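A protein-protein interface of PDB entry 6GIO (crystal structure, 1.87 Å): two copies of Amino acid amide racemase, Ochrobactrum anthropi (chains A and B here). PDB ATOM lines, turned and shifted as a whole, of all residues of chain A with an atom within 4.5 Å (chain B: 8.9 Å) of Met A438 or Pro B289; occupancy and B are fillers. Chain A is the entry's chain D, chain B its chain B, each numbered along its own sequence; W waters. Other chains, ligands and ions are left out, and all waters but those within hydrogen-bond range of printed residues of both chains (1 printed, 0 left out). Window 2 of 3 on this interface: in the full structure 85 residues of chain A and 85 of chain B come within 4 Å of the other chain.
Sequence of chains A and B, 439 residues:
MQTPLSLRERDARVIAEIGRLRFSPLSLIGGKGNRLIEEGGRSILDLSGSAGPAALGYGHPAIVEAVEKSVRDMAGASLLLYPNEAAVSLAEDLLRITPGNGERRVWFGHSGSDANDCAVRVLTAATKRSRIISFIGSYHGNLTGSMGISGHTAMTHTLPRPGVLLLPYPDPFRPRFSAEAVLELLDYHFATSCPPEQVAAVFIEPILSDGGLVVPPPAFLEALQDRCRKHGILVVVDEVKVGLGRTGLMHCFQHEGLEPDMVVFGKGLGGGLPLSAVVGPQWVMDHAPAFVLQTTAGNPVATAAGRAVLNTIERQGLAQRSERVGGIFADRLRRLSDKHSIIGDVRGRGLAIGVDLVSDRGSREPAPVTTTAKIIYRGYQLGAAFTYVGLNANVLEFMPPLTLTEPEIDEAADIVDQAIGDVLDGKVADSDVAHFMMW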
ATOM      1  N   GLU A  17       3.728 -29.695  14.482  1.00  0.00           N
ATOM      2  CA  GLU A  17       3.635 -29.235  15.875  1.00  0.00           C
ATOM      3  C   GLU A  17       2.721 -30.111  16.738  1.00  0.00           C
ATOM      4  O   GLU A  17       2.961 -30.260  17.923  1.00  0.00           O
ATOM      5  CB  GLU A  17       3.134 -27.794  15.898  1.00  0.00           C
ATOM      6  CG  GLU A  17       3.191 -27.135  17.278  1.00  0.00           C
ATOM      7  CD  GLU A  17       4.582 -26.655  17.683  1.00  0.00           C
ATOM      8  OE1 GLU A  17       5.585 -26.988  17.049  1.00  0.00           O
ATOM      9  OE2 GLU A  17       4.661 -25.882  18.646  1.00  0.00           O
ATOM     10  N   ARG A  20       4.655 -32.576  18.853  1.00  0.00           N
ATOM     11  CA  ARG A  20       5.723 -32.074  19.732  1.00  0.00           C
ATOM     12  C   ARG A  20       5.342 -31.856  21.202  1.00  0.00           C
ATOM     13  O   ARG A  20       4.270 -31.327  21.509  1.00  0.00           O
ATOM     14  CB  ARG A  20       6.157 -30.716  19.233  1.00  0.00           C
ATOM     15  CG  ARG A  20       6.924 -30.786  17.956  1.00  0.00           C
ATOM     16  CD  ARG A  20       7.617 -29.453  17.762  1.00  0.00           C
ATOM     17  NE  ARG A  20       8.400 -29.514  16.546  1.00  0.00           N
ATOM     18  CZ  ARG A  20       8.034 -28.995  15.374  1.00  0.00           C
ATOM     19  NH1 ARG A  20       6.890 -28.306  15.235  1.00  0.00           N
ATOM     20  NH2 ARG A  20       8.843 -29.140  14.339  1.00  0.00           N
ATOM     21  N   LEU A  21       6.243 -32.270  22.099  1.00  0.00           N
ATOM     22  CA  LEU A  21       6.219 -31.902  23.505  1.00  0.00           C
ATOM     23  C   LEU A  21       7.649 -31.713  23.946  1.00  0.00           C
ATOM     24  O   LEU A  21       8.246 -32.574  24.665  1.00  0.00           O
ATOM     25  CB  LEU A  21       5.563 -32.986  24.353  1.00  0.00           C
ATOM     26  CG  LEU A  21       5.317 -32.579  25.804  1.00  0.00           C
ATOM     27  CD1 LEU A  21       4.297 -31.453  25.837  1.00  0.00           C
ATOM     28  CD2 LEU A  21       4.880 -33.786  26.603  1.00  0.00           C
ATOM     29  N   MET A 437       7.523 -23.611  25.474  1.00  0.00           N
ATOM     30  CA  MET A 437       6.341 -23.367  26.289  1.00  0.00           C
ATOM     31  C   MET A 437       5.166 -23.112  25.340  1.00  0.00           C
ATOM     32  O   MET A 437       5.370 -22.738  24.203  1.00  0.00           O
ATOM     33  CB  MET A 437       6.603 -22.193  27.257  1.00  0.00           C
ATOM     34  CG  MET A 437       7.739 -22.484  28.251  1.00  0.00           C
ATOM     35  SD  MET A 437       8.042 -21.216  29.500  1.00  0.00           S
ATOM     36  CE  MET A 437       6.546 -21.301  30.462  1.00  0.00           C
ATOM     37  N   MET A 438       3.941 -23.308  25.816  1.00  0.00           N
ATOM     38  CA  MET A 438       2.748 -23.333  24.952  1.00  0.00           C
ATOM     39  C   MET A 438       1.750 -22.240  25.343  1.00  0.00           C
ATOM     40  O   MET A 438       2.106 -21.281  26.040  1.00  0.00           O
ATOM     41  CB  MET A 438       2.099 -24.725  25.043  1.00  0.00           C
ATOM     42  CG  MET A 438       3.116 -25.819  25.367  1.00  0.00           C
ATOM     43  SD  MET A 438       2.531 -27.528  25.374  1.00  0.00           S
ATOM     44  CE  MET A 438       1.825 -27.692  27.018  1.00  0.00           C
ATOM     45  N   ARG B 121      -9.177 -35.957  14.195  1.00  0.00           N
ATOM     46  CA  ARG B 121      -9.073 -35.024  15.341  1.00  0.00           C
ATOM     47  C   ARG B 121      -8.544 -33.656  14.879  1.00  0.00           C
ATOM     48  O   ARG B 121      -9.128 -32.662  15.222  1.00  0.00           O
ATOM     49  CB  ARG B 121      -8.122 -35.596  16.390  1.00  0.00           C
ATOM     50  CG  ARG B 121      -8.630 -36.840  17.100  1.00  0.00           C
ATOM     51  CD  ARG B 121      -7.881 -37.092  18.389  1.00  0.00           C
ATOM     52  NE  ARG B 121      -7.809 -35.936  19.245  1.00  0.00           N
ATOM     53  CZ  ARG B 121      -6.739 -35.540  19.902  1.00  0.00           C
ATOM     54  NH1 ARG B 121      -5.771 -36.393  20.188  1.00  0.00           N
ATOM     55  NH2 ARG B 121      -6.632 -34.276  20.246  1.00  0.00           N
ATOM     56  N   VAL B 284      -2.916 -26.742   9.112  1.00  0.00           N
ATOM     57  CA  VAL B 284      -3.600 -27.820   9.856  1.00  0.00           C
ATOM     58  C   VAL B 284      -2.653 -28.526  10.825  1.00  0.00           C
ATOM     59  O   VAL B 284      -2.990 -28.741  11.998  1.00  0.00           O
ATOM     60  CB  VAL B 284      -4.149 -28.879   8.873  1.00  0.00           C
ATOM     61  CG1 VAL B 284      -4.715 -30.100   9.609  1.00  0.00           C
ATOM     62  CG2 VAL B 284      -5.165 -28.249   7.942  1.00  0.00           C
ATOM     63  N   MET B 285      -1.480 -28.899  10.324  1.00  0.00           N
ATOM     64  CA  MET B 285      -0.597 -29.825  11.015  1.00  0.00           C
ATOM     65  C   MET B 285       0.082 -29.184  12.231  1.00  0.00           C
ATOM     66  O   MET B 285       0.434 -29.862  13.214  1.00  0.00           O
ATOM     67  CB  MET B 285       0.419 -30.413  10.035  1.00  0.00           C
ATOM     68  CG  MET B 285      -0.215 -31.194   8.912  1.00  0.00           C
ATOM     69  SD  MET B 285      -1.186 -32.642   9.441  1.00  0.00           S
ATOM     70  CE  MET B 285       0.047 -33.622  10.264  1.00  0.00           C
ATOM     71  N   ASP B 286       0.234 -27.863  12.165  1.00  0.00           N
ATOM     72  CA  ASP B 286       0.731 -27.076  13.286  1.00  0.00           C
ATOM     73  C   ASP B 286      -0.395 -26.432  14.101  1.00  0.00           C
ATOM     74  O   ASP B 286      -0.153 -25.440  14.775  1.00  0.00           O
ATOM     75  CB  ASP B 286       1.666 -25.968  12.788  1.00  0.00           C
ATOM     76  CG  ASP B 286       3.012 -26.485  12.370  1.00  0.00           C
ATOM     77  OD1 ASP B 286       3.278 -27.725  12.486  1.00  0.00           O
ATOM     78  OD2 ASP B 286       3.812 -25.625  11.902  1.00  0.00           O
ATOM     79  N   HIS B 287      -1.597 -27.005  14.077  1.00  0.00           N
ATOM     80  CA  HIS B 287      -2.793 -26.397  14.730  1.00  0.00           C
ATOM     81  C   HIS B 287      -2.528 -26.033  16.201  1.00  0.00           C
ATOM     82  O   HIS B 287      -2.858 -24.946  16.623  1.00  0.00           O
ATOM     83  CB  HIS B 287      -4.002 -27.340  14.627  1.00  0.00           C
ATOM     84  CG  HIS B 287      -5.126 -26.996  15.549  1.00  0.00           C
ATOM     85  ND1 HIS B 287      -5.962 -25.922  15.329  1.00  0.00           N
ATOM     86  CD2 HIS B 287      -5.572 -27.599  16.680  1.00  0.00           C
ATOM     87  CE1 HIS B 287      -6.860 -25.861  16.298  1.00  0.00           C
ATOM     88  NE2 HIS B 287      -6.636 -26.856  17.140  1.00  0.00           N
ATOM     89  N   ALA B 288      -1.925 -26.942  16.958  1.00  0.00           N
ATOM     90  CA  ALA B 288      -1.539 -26.650  18.329  1.00  0.00           C
ATOM     91  C   ALA B 288      -0.446 -27.594  18.789  1.00  0.00           C
ATOM     92  O   ALA B 288      -0.403 -28.733  18.356  1.00  0.00           O
ATOM     93  CB  ALA B 288      -2.744 -26.785  19.238  1.00  0.00           C
ATOM     94  N   PRO B 289       0.406 -27.149  19.726  1.00  0.00           N
ATOM     95  CA  PRO B 289       1.370 -28.091  20.230  1.00  0.00           C
ATOM     96  C   PRO B 289       0.723 -29.208  21.023  1.00  0.00           C
ATOM     97  O   PRO B 289      -0.360 -29.067  21.562  1.00  0.00           O
ATOM     98  CB  PRO B 289       2.283 -27.216  21.110  1.00  0.00           C
ATOM     99  CG  PRO B 289       1.388 -26.115  21.584  1.00  0.00           C
ATOM    100  CD  PRO B 289       0.497 -25.843  20.404  1.00  0.00           C
ATOM    101  N   ALA B 290       1.380 -30.335  21.061  1.00  0.00           N
ATOM    102  CA  ALA B 290       0.994 -31.418  21.959  1.00  0.00           C
ATOM    103  C   ALA B 290      -0.458 -31.872  21.810  1.00  0.00           C
ATOM    104  O   ALA B 290      -1.103 -32.191  22.774  1.00  0.00           O
ATOM    105  CB  ALA B 290       1.261 -31.010  23.387  1.00  0.00           C
ATOM    106  N   PHE B 291      -0.953 -31.901  20.589  1.00  0.00           N
ATOM    107  CA  PHE B 291      -2.338 -32.173  20.335  1.00  0.00           C
ATOM    108  C   PHE B 291      -2.607 -33.637  20.053  1.00  0.00           C
ATOM    109  O   PHE B 291      -3.670 -34.128  20.378  1.00  0.00           O
ATOM    110  CB  PHE B 291      -2.755 -31.360  19.132  1.00  0.00           C
ATOM    111  CG  PHE B 291      -4.233 -31.272  18.940  1.00  0.00           C
ATOM    112  CD1 PHE B 291      -5.046 -30.730  19.933  1.00  0.00           C
ATOM    113  CD2 PHE B 291      -4.807 -31.664  17.740  1.00  0.00           C
ATOM    114  CE1 PHE B 291      -6.406 -30.620  19.747  1.00  0.00           C
ATOM    115  CE2 PHE B 291      -6.164 -31.575  17.541  1.00  0.00           C
ATOM    116  CZ  PHE B 291      -6.971 -31.049  18.546  1.00  0.00           C
ATOM    117  N   VAL B 292      -1.675 -34.308  19.385  1.00  0.00           N
ATOM    118  CA  VAL B 292      -1.798 -35.741  19.139  1.00  0.00           C
ATOM    119  C   VAL B 292      -0.465 -36.418  19.447  1.00  0.00           C
ATOM    120  O   VAL B 292       0.387 -36.524  18.585  1.00  0.00           O
ATOM    121  CB  VAL B 292      -2.250 -36.048  17.697  1.00  0.00           C
ATOM    122  CG1 VAL B 292      -2.667 -37.505  17.593  1.00  0.00           C
ATOM    123  CG2 VAL B 292      -3.434 -35.173  17.284  1.00  0.00           C
ATOM    124  N   LEU B 293      -0.317 -36.895  20.685  1.00  0.00           N
ATOM    125  CA  LEU B 293       0.939 -37.401  21.207  1.00  0.00           C
ATOM    126  C   LEU B 293       0.903 -38.884  21.444  1.00  0.00           C
ATOM    127  O   LEU B 293      -0.068 -39.407  22.024  1.00  0.00           O
ATOM    128  CB  LEU B 293       1.233 -36.768  22.554  1.00  0.00           C
ATOM    129  CG  LEU B 293       1.476 -35.253  22.615  1.00  0.00           C
ATOM    130  CD1 LEU B 293       1.935 -34.909  24.030  1.00  0.00           C
ATOM    131  CD2 LEU B 293       2.485 -34.797  21.580  1.00  0.00           C
HETATM  132  O   HOH W   1       6.110 -27.404  12.301  1.00  0.00           O
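The backbone NH (N) of Glu A17 sits at hydrogen-bond distance from the side-chain carboxylate (OD1) of Asp B286, at 2.8 Å.
The backbone carbonyl oxygen (O) of Arg A20 sits at hydrogen-bond distance from the backbone NH (N) of Ala B290 (3.1 Å).
The side-chain carboxylate of Glu A17 lies within salt-bridge range of the guanidinium group of Arg A20 (2.6 Å).
Among the printed residues, merely in contact across the chains: Glu A17 with Met B285, Glu A17 with Ala B288, Glu A17 with Pro B289, Glu A17 with Ala B290, Arg A20 with Leu B293, Leu A21 with Ala B290 and Met A438 with Pro B289.
Printed residues of chain B within 4 Å of Glu A17: Met B285 (3.5 Å), Asp B286 (2.8 Å), Ala B288 (3.7 Å), Pro B289 (3.5 Å) and Ala B290 (3.5 Å).
Met A437 touches none of the printed residues of chain B.
Printed residues of chain B within 4 Å of Met A438: Pro B289.
Of the printed residues of chain A, Met B285 touches Glu A17.
Of chain A, only Glu A17 and Met A438 come within 4 Å of Pro B289.
The nearest residue of chain A that does not touch Pro B289 is Arg A20 (4.2 Å).
The nearest printed residue of chain B that does not touch Leu A21 is Leu B293 (4.1 Å).
Hydrophobic or aromatic side chains of chain A that line the printed part of chain B: Leu A21 and Met A438.
Hydrophobic or aromatic side chains of chain B within 4 Å of the printed part of chain A: Pro B289, Ala B290 and Leu B293.
Among the printed residues, 9 pairs touch across the chains.
Among the printed residues, no Asp or Glu carboxylate lies within 4 Å of a Lys or Arg side-chain nitrogen of the other chain.
No position is printed for both chains.
Water W1 bridges OD1 of Asp B286 (2.9 Å) and NH1 of Arg A20 (3.2 Å).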
